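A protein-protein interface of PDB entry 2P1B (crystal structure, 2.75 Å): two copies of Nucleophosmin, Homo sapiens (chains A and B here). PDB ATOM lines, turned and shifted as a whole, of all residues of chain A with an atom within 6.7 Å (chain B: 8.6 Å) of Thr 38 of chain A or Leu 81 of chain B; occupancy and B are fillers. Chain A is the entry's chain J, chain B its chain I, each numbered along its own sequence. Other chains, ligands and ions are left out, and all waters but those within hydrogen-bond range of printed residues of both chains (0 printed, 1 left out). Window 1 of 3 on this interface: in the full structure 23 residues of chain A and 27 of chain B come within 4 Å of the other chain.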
ATOM      1  N   LEU A  36      11.765  24.530 -19.136  1.00  0.00           N
ATOM      2  CA  LEU A  36      10.308  24.583 -19.127  1.00  0.00           C
ATOM      3  C   LEU A  36       9.673  24.082 -17.839  1.00  0.00           C
ATOM      4  O   LEU A  36      10.077  23.063 -17.273  1.00  0.00           O
ATOM      5  CB  LEU A  36       9.754  23.804 -20.317  1.00  0.00           C
ATOM      6  CG  LEU A  36      10.127  24.468 -21.642  1.00  0.00           C
ATOM      7  CD1 LEU A  36       9.730  23.604 -22.825  1.00  0.00           C
ATOM      8  CD2 LEU A  36       9.446  25.815 -21.700  1.00  0.00           C
ATOM      9  N   ARG A  37       8.675  24.821 -17.372  1.00  0.00           N
ATOM     10  CA  ARG A  37       7.978  24.458 -16.154  1.00  0.00           C
ATOM     11  C   ARG A  37       6.600  23.893 -16.443  1.00  0.00           C
ATOM     12  O   ARG A  37       6.464  22.718 -16.781  1.00  0.00           O
ATOM     13  CB  ARG A  37       7.893  25.666 -15.221  1.00  0.00           C
ATOM     14  CG  ARG A  37       9.195  25.892 -14.468  1.00  0.00           C
ATOM     15  CD  ARG A  37       9.332  24.846 -13.398  1.00  0.00           C
ATOM     16  NE  ARG A  37      10.691  24.351 -13.212  1.00  0.00           N
ATOM     17  CZ  ARG A  37      11.030  23.532 -12.222  1.00  0.00           C
ATOM     18  NH1 ARG A  37      10.112  23.138 -11.347  1.00  0.00           N
ATOM     19  NH2 ARG A  37      12.274  23.097 -12.105  1.00  0.00           N
ATOM     20  N   THR A  38       5.569  24.710 -16.332  1.00  0.00           N
ATOM     21  CA  THR A  38       4.248  24.185 -16.583  1.00  0.00           C
ATOM     22  C   THR A  38       3.639  24.611 -17.903  1.00  0.00           C
ATOM     23  O   THR A  38       3.995  25.651 -18.461  1.00  0.00           O
ATOM     24  CB  THR A  38       3.303  24.556 -15.438  1.00  0.00           C
ATOM     25  OG1 THR A  38       3.100  25.976 -15.422  1.00  0.00           O
ATOM     26  CG2 THR A  38       3.903  24.102 -14.111  1.00  0.00           C
ATOM     27  N   VAL A  39       2.723  23.775 -18.390  1.00  0.00           N
ATOM     28  CA  VAL A  39       1.990  23.995 -19.636  1.00  0.00           C
ATOM     29  C   VAL A  39       0.515  23.974 -19.254  1.00  0.00           C
ATOM     30  O   VAL A  39       0.051  23.021 -18.632  1.00  0.00           O
ATOM     31  CB  VAL A  39       2.240  22.860 -20.621  1.00  0.00           C
ATOM     32  CG1 VAL A  39       1.718  23.251 -21.987  1.00  0.00           C
ATOM     33  CG2 VAL A  39       3.722  22.516 -20.651  1.00  0.00           C
ATOM     34  N   SER A  40      -0.224  25.015 -19.615  1.00  0.00           N
ATOM     35  CA  SER A  40      -1.636  25.065 -19.242  1.00  0.00           C
ATOM     36  C   SER A  40      -2.539  25.828 -20.206  1.00  0.00           C
ATOM     37  O   SER A  40      -2.177  26.904 -20.682  1.00  0.00           O
ATOM     38  CB  SER A  40      -1.769  25.664 -17.844  1.00  0.00           C
ATOM     39  OG  SER A  40      -1.056  26.878 -17.757  1.00  0.00           O
ATOM     40  N   THR A  78      -3.532  21.134 -17.250  1.00  0.00           N
ATOM     41  CA  THR A  78      -2.144  21.491 -16.976  1.00  0.00           C
ATOM     42  C   THR A  78      -1.202  20.324 -16.744  1.00  0.00           C
ATOM     43  O   THR A  78      -1.460  19.449 -15.912  1.00  0.00           O
ATOM     44  CB  THR A  78      -2.019  22.395 -15.735  1.00  0.00           C
ATOM     45  OG1 THR A  78      -2.811  23.577 -15.903  1.00  0.00           O
ATOM     46  CG2 THR A  78      -0.564  22.794 -15.523  1.00  0.00           C
ATOM     47  N   VAL A  79      -0.096  20.332 -17.480  1.00  0.00           N
ATOM     48  CA  VAL A  79       0.933  19.309 -17.348  1.00  0.00           C
ATOM     49  C   VAL A  79       2.137  20.048 -16.797  1.00  0.00           C
ATOM     50  O   VAL A  79       2.413  21.169 -17.203  1.00  0.00           O
ATOM     51  CB  VAL A  79       1.297  18.684 -18.712  1.00  0.00           C
ATOM     52  CG1 VAL A  79       2.498  17.793 -18.562  1.00  0.00           C
ATOM     53  CG2 VAL A  79       0.107  17.899 -19.265  1.00  0.00           C
ATOM     54  N   SER A  80       2.835  19.443 -15.849  1.00  0.00           N
ATOM     55  CA  SER A  80       4.009  20.091 -15.285  1.00  0.00           C
ATOM     56  C   SER A  80       5.240  19.251 -15.606  1.00  0.00           C
ATOM     57  O   SER A  80       5.312  18.072 -15.269  1.00  0.00           O
ATOM     58  CB  SER A  80       3.855  20.267 -13.773  1.00  0.00           C
ATOM     59  OG  SER A  80       4.972  20.953 -13.239  1.00  0.00           O
ATOM     60  N   LEU A  81       6.207  19.865 -16.272  1.00  0.00           N
ATOM     61  CA  LEU A  81       7.421  19.176 -16.669  1.00  0.00           C
ATOM     62  C   LEU A  81       8.509  19.342 -15.621  1.00  0.00           C
ATOM     63  O   LEU A  81       9.500  18.616 -15.624  1.00  0.00           O
ATOM     64  CB  LEU A  81       7.898  19.732 -17.998  1.00  0.00           C
ATOM     65  CG  LEU A  81       6.761  20.034 -18.971  1.00  0.00           C
ATOM     66  CD1 LEU A  81       7.304  20.799 -20.179  1.00  0.00           C
ATOM     67  CD2 LEU A  81       6.080  18.729 -19.376  1.00  0.00           C
ATOM     68  N   GLY A  82       8.324  20.316 -14.737  1.00  0.00           N
ATOM     69  CA  GLY A  82       9.289  20.549 -13.681  1.00  0.00           C
ATOM     70  C   GLY A  82      10.761  20.593 -14.057  1.00  0.00           C
ATOM     71  O   GLY A  82      11.530  19.686 -13.730  1.00  0.00           O
ATOM     72  N   GLY A  83      11.161  21.659 -14.737  1.00  0.00           N
ATOM     73  CA  GLY A  83      12.552  21.797 -15.109  1.00  0.00           C
ATOM     74  C   GLY A  83      13.008  20.911 -16.241  1.00  0.00           C
ATOM     75  O   GLY A  83      13.894  20.078 -16.077  1.00  0.00           O
ATOM     76  N   HIS A 102      -0.617  28.328 -22.360  1.00  0.00           N
ATOM     77  CA  HIS A 102       0.355  29.079 -21.578  1.00  0.00           C
ATOM     78  C   HIS A 102       1.543  28.217 -21.142  1.00  0.00           C
ATOM     79  O   HIS A 102       1.370  27.177 -20.490  1.00  0.00           O
ATOM     80  CB  HIS A 102      -0.323  29.678 -20.335  1.00  0.00           C
ATOM     81  CG  HIS A 102      -1.131  30.904 -20.618  1.00  0.00           C
ATOM     82  ND1 HIS A 102      -0.565  32.154 -20.761  1.00  0.00           N
ATOM     83  CD2 HIS A 102      -2.461  31.074 -20.808  1.00  0.00           C
ATOM     84  CE1 HIS A 102      -1.510  33.037 -21.026  1.00  0.00           C
ATOM     85  NE2 HIS A 102      -2.670  32.408 -21.061  1.00  0.00           N
ATOM     86  N   ILE A 103       2.745  28.644 -21.520  1.00  0.00           N
ATOM     87  CA  ILE A 103       3.955  27.938 -21.122  1.00  0.00           C
ATOM     88  C   ILE A 103       4.739  28.851 -20.202  1.00  0.00           C
ATOM     89  O   ILE A 103       4.980  30.015 -20.524  1.00  0.00           O
ATOM     90  CB  ILE A 103       4.841  27.557 -22.320  1.00  0.00           C
ATOM     91  CG1 ILE A 103       4.021  26.736 -23.326  1.00  0.00           C
ATOM     92  CG2 ILE A 103       6.056  26.794 -21.826  1.00  0.00           C
ATOM     93  CD1 ILE A 103       4.829  25.821 -24.213  1.00  0.00           C
ATOM     94  N   SER A 104       5.105  28.328 -19.038  1.00  0.00           N
ATOM     95  CA  SER A 104       5.858  29.093 -18.049  1.00  0.00           C
ATOM     96  C   SER A 104       7.152  28.357 -17.840  1.00  0.00           C
ATOM     97  O   SER A 104       7.202  27.141 -17.982  1.00  0.00           O
ATOM     98  CB  SER A 104       5.109  29.152 -16.721  1.00  0.00           C
ATOM     99  OG  SER A 104       5.109  27.881 -16.093  1.00  0.00           O
ATOM    100  N   GLY A 105       8.199  29.083 -17.487  1.00  0.00           N
ATOM    101  CA  GLY A 105       9.467  28.420 -17.299  1.00  0.00           C
ATOM    102  C   GLY A 105      10.558  29.366 -16.877  1.00  0.00           C
ATOM    103  O   GLY A 105      10.281  30.418 -16.301  1.00  0.00           O
ATOM    104  N   SER B  35      11.185  29.783  -4.444  1.00  0.00           N
ATOM    105  CA  SER B  35      10.868  28.490  -5.048  1.00  0.00           C
ATOM    106  C   SER B  35       9.427  28.055  -4.784  1.00  0.00           C
ATOM    107  O   SER B  35       9.089  27.630  -3.680  1.00  0.00           O
ATOM    108  CB  SER B  35      11.840  27.430  -4.520  1.00  0.00           C
ATOM    109  OG  SER B  35      11.688  26.202  -5.209  1.00  0.00           O
ATOM    110  N   LEU B  36       8.584  28.151  -5.807  1.00  0.00           N
ATOM    111  CA  LEU B  36       7.177  27.776  -5.686  1.00  0.00           C
ATOM    112  C   LEU B  36       6.987  26.265  -5.706  1.00  0.00           C
ATOM    113  O   LEU B  36       7.703  25.559  -6.405  1.00  0.00           O
ATOM    114  CB  LEU B  36       6.377  28.415  -6.819  1.00  0.00           C
ATOM    115  CG  LEU B  36       6.412  29.945  -6.781  1.00  0.00           C
ATOM    116  CD1 LEU B  36       5.743  30.532  -8.028  1.00  0.00           C
ATOM    117  CD2 LEU B  36       5.733  30.412  -5.499  1.00  0.00           C
ATOM    118  N   ARG B  37       6.021  25.769  -4.938  1.00  0.00           N
ATOM    119  CA  ARG B  37       5.760  24.330  -4.892  1.00  0.00           C
ATOM    120  C   ARG B  37       4.414  23.947  -5.490  1.00  0.00           C
ATOM    121  O   ARG B  37       4.346  23.484  -6.634  1.00  0.00           O
ATOM    122  CB  ARG B  37       5.859  23.819  -3.451  1.00  0.00           C
ATOM    123  CG  ARG B  37       7.288  23.649  -2.972  1.00  0.00           C
ATOM    124  CD  ARG B  37       7.905  22.422  -3.612  1.00  0.00           C
ATOM    125  NE  ARG B  37       9.357  22.509  -3.718  1.00  0.00           N
ATOM    126  CZ  ARG B  37      10.119  21.555  -4.243  1.00  0.00           C
ATOM    127  NH1 ARG B  37       9.562  20.442  -4.705  1.00  0.00           N
ATOM    128  NH2 ARG B  37      11.432  21.719  -4.316  1.00  0.00           N
ATOM    129  N   THR B  38       3.342  24.150  -4.731  1.00  0.00           N
ATOM    130  CA  THR B  38       2.017  23.798  -5.214  1.00  0.00           C
ATOM    131  C   THR B  38       1.057  24.966  -5.309  1.00  0.00           C
ATOM    132  O   THR B  38       1.088  25.882  -4.492  1.00  0.00           O
ATOM    133  CB  THR B  38       1.343  22.752  -4.315  1.00  0.00           C
ATOM    134  OG1 THR B  38       1.050  23.343  -3.046  1.00  0.00           O
ATOM    135  CG2 THR B  38       2.243  21.554  -4.111  1.00  0.00           C
ATOM    136  N   VAL B  39       0.209  24.909  -6.331  1.00  0.00           N
ATOM    137  CA  VAL B  39      -0.833  25.894  -6.566  1.00  0.00           C
ATOM    138  C   VAL B  39      -2.113  25.080  -6.390  1.00  0.00           C
ATOM    139  O   VAL B  39      -2.277  24.031  -7.016  1.00  0.00           O
ATOM    140  CB  VAL B  39      -0.790  26.439  -7.992  1.00  0.00           C
ATOM    141  CG1 VAL B  39      -1.869  27.485  -8.174  1.00  0.00           C
ATOM    142  CG2 VAL B  39       0.577  27.019  -8.279  1.00  0.00           C
ATOM    143  N   SER B  40      -3.011  25.545  -5.534  1.00  0.00           N
ATOM    144  CA  SER B  40      -4.239  24.808  -5.282  1.00  0.00           C
ATOM    145  C   SER B  40      -5.431  25.680  -4.874  1.00  0.00           C
ATOM    146  O   SER B  40      -5.265  26.778  -4.344  1.00  0.00           O
ATOM    147  CB  SER B  40      -3.968  23.736  -4.216  1.00  0.00           C
ATOM    148  OG  SER B  40      -2.861  24.095  -3.402  1.00  0.00           O
ATOM    149  N   VAL B  52      -3.483  31.036 -12.590  1.00  0.00           N
ATOM    150  CA  VAL B  52      -2.586  31.746 -11.704  1.00  0.00           C
ATOM    151  C   VAL B  52      -1.365  32.181 -12.504  1.00  0.00           C
ATOM    152  O   VAL B  52      -0.673  31.344 -13.089  1.00  0.00           O
ATOM    153  CB  VAL B  52      -2.138  30.850 -10.533  1.00  0.00           C
ATOM    154  CG1 VAL B  52      -1.164  31.617  -9.635  1.00  0.00           C
ATOM    155  CG2 VAL B  52      -3.358  30.382  -9.744  1.00  0.00           C
ATOM    156  N   ALA B  54       2.270  34.716 -12.633  1.00  0.00           N
ATOM    157  CA  ALA B  54       3.294  35.343 -11.804  1.00  0.00           C
ATOM    158  C   ALA B  54       4.020  36.473 -12.510  1.00  0.00           C
ATOM    159  O   ALA B  54       4.212  36.434 -13.731  1.00  0.00           O
ATOM    160  CB  ALA B  54       4.301  34.295 -11.353  1.00  0.00           C
ATOM    161  N   VAL B  66       3.503  35.731 -16.339  1.00  0.00           N
ATOM    162  CA  VAL B  66       3.588  34.347 -16.759  1.00  0.00           C
ATOM    163  C   VAL B  66       2.555  33.473 -16.064  1.00  0.00           C
ATOM    164  O   VAL B  66       2.196  33.738 -14.928  1.00  0.00           O
ATOM    165  CB  VAL B  66       5.005  33.840 -16.447  1.00  0.00           C
ATOM    166  CG1 VAL B  66       4.980  32.377 -16.070  1.00  0.00           C
ATOM    167  CG2 VAL B  66       5.904  34.094 -17.640  1.00  0.00           C
ATOM    168  N   THR B  67       2.091  32.424 -16.735  1.00  0.00           N
ATOM    169  CA  THR B  67       1.107  31.537 -16.126  1.00  0.00           C
ATOM    170  C   THR B  67       1.707  30.356 -15.357  1.00  0.00           C
ATOM    171  O   THR B  67       2.397  29.519 -15.920  1.00  0.00           O
ATOM    172  CB  THR B  67       0.152  30.978 -17.174  1.00  0.00           C
ATOM    173  OG1 THR B  67      -0.356  32.049 -17.976  1.00  0.00           O
ATOM    174  CG2 THR B  67      -1.010  30.275 -16.489  1.00  0.00           C
ATOM    175  N   LEU B  68       1.435  30.283 -14.065  1.00  0.00           N
ATOM    176  CA  LEU B  68       1.959  29.187 -13.272  1.00  0.00           C
ATOM    177  C   LEU B  68       1.093  27.946 -13.400  1.00  0.00           C
ATOM    178  O   LEU B  68       1.589  26.829 -13.280  1.00  0.00           O
ATOM    179  CB  LEU B  68       2.064  29.595 -11.806  1.00  0.00           C
ATOM    180  CG  LEU B  68       3.086  30.693 -11.511  1.00  0.00           C
ATOM    181  CD1 LEU B  68       3.185  30.890 -10.009  1.00  0.00           C
ATOM    182  CD2 LEU B  68       4.427  30.309 -12.072  1.00  0.00           C
ATOM    183  N   ALA B  69      -0.199  28.140 -13.658  1.00  0.00           N
ATOM    184  CA  ALA B  69      -1.110  27.010 -13.789  1.00  0.00           C
ATOM    185  C   ALA B  69      -2.565  27.375 -14.075  1.00  0.00           C
ATOM    186  O   ALA B  69      -3.013  28.488 -13.807  1.00  0.00           O
ATOM    187  CB  ALA B  69      -1.047  26.156 -12.526  1.00  0.00           C
ATOM    188  N   THR B  70      -3.292  26.405 -14.621  1.00  0.00           N
ATOM    189  CA  THR B  70      -4.708  26.546 -14.917  1.00  0.00           C
ATOM    190  C   THR B  70      -5.392  25.459 -14.093  1.00  0.00           C
ATOM    191  O   THR B  70      -5.224  24.272 -14.356  1.00  0.00           O
ATOM    192  CB  THR B  70      -4.986  26.329 -16.406  1.00  0.00           C
ATOM    193  OG1 THR B  70      -4.499  27.456 -17.138  1.00  0.00           O
ATOM    194  CG2 THR B  70      -6.476  26.167 -16.661  1.00  0.00           C
ATOM    195  N   THR B  78      -5.219  20.854  -7.843  1.00  0.00           N
ATOM    196  CA  THR B  78      -3.841  21.165  -7.495  1.00  0.00           C
ATOM    197  C   THR B  78      -2.831  20.900  -8.588  1.00  0.00           C
ATOM    198  O   THR B  78      -2.915  19.907  -9.306  1.00  0.00           O
ATOM    199  CB  THR B  78      -3.395  20.358  -6.261  1.00  0.00           C
ATOM    200  OG1 THR B  78      -4.170  20.747  -5.119  1.00  0.00           O
ATOM    201  CG2 THR B  78      -1.917  20.594  -5.976  1.00  0.00           C
ATOM    202  N   VAL B  79      -1.870  21.808  -8.701  1.00  0.00           N
ATOM    203  CA  VAL B  79      -0.795  21.677  -9.672  1.00  0.00           C
ATOM    204  C   VAL B  79       0.495  21.776  -8.872  1.00  0.00           C
ATOM    205  O   VAL B  79       0.657  22.684  -8.049  1.00  0.00           O
ATOM    206  CB  VAL B  79      -0.825  22.803 -10.724  1.00  0.00           C
ATOM    207  CG1 VAL B  79       0.358  22.661 -11.661  1.00  0.00           C
ATOM    208  CG2 VAL B  79      -2.112  22.748 -11.519  1.00  0.00           C
ATOM    209  N   SER B  80       1.404  20.832  -9.095  1.00  0.00           N
ATOM    210  CA  SER B  80       2.676  20.818  -8.385  1.00  0.00           C
ATOM    211  C   SER B  80       3.823  21.252  -9.299  1.00  0.00           C
ATOM    212  O   SER B  80       4.342  20.462 -10.091  1.00  0.00           O
ATOM    213  CB  SER B  80       2.950  19.418  -7.828  1.00  0.00           C
ATOM    214  OG  SER B  80       4.114  19.397  -7.021  1.00  0.00           O
ATOM    215  N   LEU B  81       4.218  22.517  -9.168  1.00  0.00           N
ATOM    216  CA  LEU B  81       5.294  23.101  -9.965  1.00  0.00           C
ATOM    217  C   LEU B  81       6.654  22.534  -9.563  1.00  0.00           C
ATOM    218  O   LEU B  81       7.627  22.631 -10.308  1.00  0.00           O
ATOM    219  CB  LEU B  81       5.293  24.615  -9.780  1.00  0.00           C
ATOM    220  CG  LEU B  81       3.949  25.302 -10.032  1.00  0.00           C
ATOM    221  CD1 LEU B  81       3.810  26.533  -9.153  1.00  0.00           C
ATOM    222  CD2 LEU B  81       3.835  25.660 -11.493  1.00  0.00           C
ATOM    223  N   GLY B  82       6.706  21.959  -8.366  1.00  0.00           N
ATOM    224  CA  GLY B  82       7.926  21.357  -7.859  1.00  0.00           C
ATOM    225  C   GLY B  82       9.200  22.181  -7.860  1.00  0.00           C
ATOM    226  O   GLY B  82      10.162  21.834  -8.547  1.00  0.00           O
ATOM    227  N   GLY B  83       9.216  23.265  -7.090  1.00  0.00           N
ATOM    228  CA  GLY B  83      10.406  24.096  -7.005  1.00  0.00           C
ATOM    229  C   GLY B  83      10.725  24.990  -8.188  1.00  0.00           C
ATOM    230  O   GLY B  83      11.825  24.942  -8.732  1.00  0.00           O
ATOM    231  N   PHE B  84       9.756  25.802  -8.591  1.00  0.00           N
ATOM    232  CA  PHE B  84       9.922  26.750  -9.687  1.00  0.00           C
ATOM    233  C   PHE B  84      10.518  27.964  -8.972  1.00  0.00           C
ATOM    234  O   PHE B  84       9.818  28.669  -8.245  1.00  0.00           O
ATOM    235  CB  PHE B  84       8.537  27.063 -10.287  1.00  0.00           C
ATOM    236  CG  PHE B  84       8.554  27.903 -11.556  1.00  0.00           C
ATOM    237  CD1 PHE B  84       7.519  27.775 -12.492  1.00  0.00           C
ATOM    238  CD2 PHE B  84       9.532  28.863 -11.783  1.00  0.00           C
ATOM    239  CE1 PHE B  84       7.452  28.593 -13.627  1.00  0.00           C
ATOM    240  CE2 PHE B  84       9.473  29.688 -12.919  1.00  0.00           C
ATOM    241  CZ  PHE B  84       8.427  29.550 -13.840  1.00  0.00           C
ATOM    242  N   GLU B  85      11.822  28.173  -9.134  1.00  0.00           N
ATOM    243  CA  GLU B  85      12.500  29.301  -8.501  1.00  0.00           C
ATOM    244  C   GLU B  85      12.391  30.570  -9.350  1.00  0.00           C
ATOM    245  O   GLU B  85      12.682  30.565 -10.547  1.00  0.00           O
ATOM    246  CB  GLU B  85      13.971  28.967  -8.261  1.00  0.00           C
ATOM    247  CG  GLU B  85      14.253  28.081  -7.051  1.00  0.00           C
ATOM    248  CD  GLU B  85      15.606  27.374  -7.147  1.00  0.00           C
ATOM    249  OE1 GLU B  85      15.677  26.305  -7.793  1.00  0.00           O
ATOM    250  OE2 GLU B  85      16.601  27.890  -6.593  1.00  0.00           O
ATOM    251  N   ILE B  86      11.959  31.654  -8.717  1.00  0.00           N
ATOM    252  CA  ILE B  86      11.801  32.942  -9.382  1.00  0.00           C
ATOM    253  C   ILE B  86      12.538  33.999  -8.561  1.00  0.00           C
ATOM    254  O   ILE B  86      12.441  34.016  -7.325  1.00  0.00           O
ATOM    255  CB  ILE B  86      10.317  33.326  -9.498  1.00  0.00           C
ATOM    256  CG1 ILE B  86       9.537  32.179 -10.134  1.00  0.00           C
ATOM    257  CG2 ILE B  86      10.165  34.558 -10.356  1.00  0.00           C
ATOM    258  CD1 ILE B  86       8.104  32.521 -10.483  1.00  0.00           C
ATOM    259  N   LEU B  92       2.305  37.528  -7.416  1.00  0.00           N
ATOM    260  CA  LEU B  92       1.465  36.400  -7.777  1.00  0.00           C
ATOM    261  C   LEU B  92       0.007  36.862  -7.818  1.00  0.00           C
ATOM    262  O   LEU B  92      -0.462  37.553  -6.912  1.00  0.00           O
ATOM    263  CB  LEU B  92       1.666  35.292  -6.746  1.00  0.00           C
ATOM    264  CG  LEU B  92       3.149  34.993  -6.487  1.00  0.00           C
ATOM    265  CD1 LEU B  92       3.360  34.547  -5.042  1.00  0.00           C
ATOM    266  CD2 LEU B  92       3.644  33.953  -7.490  1.00  0.00           C
ATOM    267  N   HIS B 102      -4.582  28.953  -3.029  1.00  0.00           N
ATOM    268  CA  HIS B 102      -3.413  28.912  -2.148  1.00  0.00           C
ATOM    269  C   HIS B 102      -2.133  28.557  -2.926  1.00  0.00           C
ATOM    270  O   HIS B 102      -2.182  27.819  -3.911  1.00  0.00           O
ATOM    271  CB  HIS B 102      -3.633  27.874  -1.041  1.00  0.00           C
ATOM    272  CG  HIS B 102      -4.924  28.032  -0.299  1.00  0.00           C
ATOM    273  ND1 HIS B 102      -5.097  28.946   0.719  1.00  0.00           N
ATOM    274  CD2 HIS B 102      -6.106  27.384  -0.424  1.00  0.00           C
ATOM    275  CE1 HIS B 102      -6.328  28.850   1.190  1.00  0.00           C
ATOM    276  NE2 HIS B 102      -6.960  27.908   0.513  1.00  0.00           N
ATOM    277  N   ILE B 103      -0.995  29.084  -2.470  1.00  0.00           N
ATOM    278  CA  ILE B 103       0.311  28.831  -3.098  1.00  0.00           C
ATOM    279  C   ILE B 103       1.398  28.565  -2.048  1.00  0.00           C
ATOM    280  O   ILE B 103       1.687  29.420  -1.219  1.00  0.00           O
ATOM    281  CB  ILE B 103       0.747  30.030  -3.986  1.00  0.00           C
ATOM    282  CG1 ILE B 103      -0.146  30.105  -5.224  1.00  0.00           C
ATOM    283  CG2 ILE B 103       2.197  29.886  -4.403  1.00  0.00           C
ATOM    284  CD1 ILE B 103       0.239  31.201  -6.165  1.00  0.00           C
ATOM    285  N   SER B 104       1.990  27.374  -2.076  1.00  0.00           N
ATOM    286  CA  SER B 104       3.029  27.030  -1.108  1.00  0.00           C
ATOM    287  C   SER B 104       4.382  27.056  -1.780  1.00  0.00           C
ATOM    288  O   SER B 104       4.483  27.061  -3.011  1.00  0.00           O
ATOM    289  CB  SER B 104       2.800  25.634  -0.517  1.00  0.00           C
ATOM    290  OG  SER B 104       3.251  24.607  -1.384  1.00  0.00           O
ATOM    291  N   GLY B 105       5.428  27.064  -0.967  1.00  0.00           N
ATOM    292  CA  GLY B 105       6.761  27.092  -1.523  1.00  0.00           C
ATOM    293  C   GLY B 105       7.822  27.356  -0.481  1.00  0.00           C
ATOM    294  O   GLY B 105       7.596  27.148   0.712  1.00  0.00           O
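The side-chain hydroxyl (OG1) of Thr 67 of chain B is in hydrogen-bond range of a ring nitrogen (ND1) of His 102 of chain A (2.8 Å).
OG of Ser 104 of chain A lies close to O of Thr 67 of chain B (3.2 Å).
The backbone carbonyl oxygen of Leu 68 of chain B sits at hydrogen-bond distance from the side-chain hydroxyl of Thr 38 of chain A, 2.8 Å away.
The backbone carbonyl oxygen of Thr 70 of chain B lies within hydrogen-bond range of the side-chain hydroxyl of Thr 78 of chain A (2.9 Å).
The backbone carbonyl oxygen (O) of Ser 80 of chain B is in hydrogen-bond range of the side-chain hydroxyl (OG) of Ser 80 of chain A, 3.2 Å away.
The backbone carbonyl oxygen (O) of Leu 81 of chain B is in hydrogen-bond range of the guanidinium group (NH1) of Arg 37 of chain A, at 2.7 Å.
The guanidinium group (NH1) of Arg 37 of chain A lies within hydrogen-bond range of the backbone carbonyl oxygen (O) of Gly 82 of chain B.
The backbone carbonyl oxygen of Arg 37 of chain B lies within hydrogen-bond range of the backbone NH of Gly 82 of chain B.
The backbone carbonyl oxygen (O) of Val 39 of chain B lies within hydrogen-bond range of the backbone NH (N) of Val 79 of chain B, at 2.8 Å.
The backbone carbonyl oxygen (O) of Val 52 of chain B sits at hydrogen-bond distance from the backbone NH (N) of Leu 68 of chain B.
N of Leu 81 of chain A sits at hydrogen-bond distance from O of Arg 37 of chain A.
OG of Ser 104 of chain A is in hydrogen-bond range of OG1 of Thr 38 of chain A (2.8 Å).
The backbone NH of His 102 of chain A lies within hydrogen-bond range of the backbone carbonyl oxygen of Ser 40 of chain A (2.7 Å).
O of Gly 83 of chain B touches NH1 of Arg 37 of chain A (3.6 Å).
Arg 37 of chain A touches Phe 84 of chain B (CG to CD1, 3.2 Å).
Thr 38 of chain A touches Leu 81 of chain B (CG2 to CD2, 3.0 Å).
Thr 67 of chain B touches Ser 40 of chain A.
Ser 40 of chain A touches Ala 69 of chain B.
Ser 40 of chain A touches Thr 70 of chain B (CB to OG1, 3.3 Å).
Thr 78 of chain A touches Val 79 of chain B.
Leu 81 of chain B touches Ser 80 of chain A.
Val 66 of chain B touches Ser 104 of chain A.
OG of Ser 104 of chain A touches CE1 of Phe 84 of chain B (3.5 Å).
Ser 104 of chain A touches just these residues of chain B: Val 66 (3.3 Å), Thr 67 (2.9 Å) and Phe 84 (3.5 Å).
Of the printed residues of chain A, Leu 68 of chain B touches Thr 38 (2.8 Å).
Of the printed residues of chain A, Thr 70 of chain B touches Ser 40 (3.3 Å) and Thr 78 (2.9 Å).
Leu 81 of chain B touches three residues of chain A.
Printed residues of chain A within 4 Å of Phe 84 of chain B: Arg 37, Ser 104 and Gly 105.
The nearest residue of chain B that does not touch Thr 38 of chain A is Ala 69 of chain B (4.3 Å).
The nearest residue of chain A that does not touch Leu 81 of chain B is Gly 82 of chain A (4.3 Å).
The nearest printed residue of chain B that does not touch Arg 37 of chain A is Glu 85 of chain B (5.6 Å).
Printed residues of chain B that touch a printed residue of chain A: Val 66, Thr 67, Leu 68, Ala 69, Thr 70, Val 79, Ser 80, Leu 81, Gly 82, Gly 83 and Phe 84.
Hydrophobic or aromatic side chains of chain A that line the printed part of chain B: His 102.
Among the printed residues, 19 pairs touch across the chains.
Arg 37 of chain A touches Leu 81 of chain B, but with the chains exchanged Leu 81 of chain A does not touch Arg 37 of chain B (10.5 Å).
Thr 38 of chain A touches Leu 81 of chain B, but with the chains exchanged Leu 81 of chain A does not touch Thr 38 of chain B (12.5 Å).
Ser 80 of chain B touches its own counterpart, Ser 80 of chain A.
Ser 80 of chain A touches Leu 81 of chain B, but with the chains exchanged Leu 81 of chain A does not touch Ser 80 of chain B (6.5 Å).
Positions printed for both chains: 36, 37, 38, 39, 40, 78, 79, 80, 81, 82, 83, 102, 103, 104 and 105.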
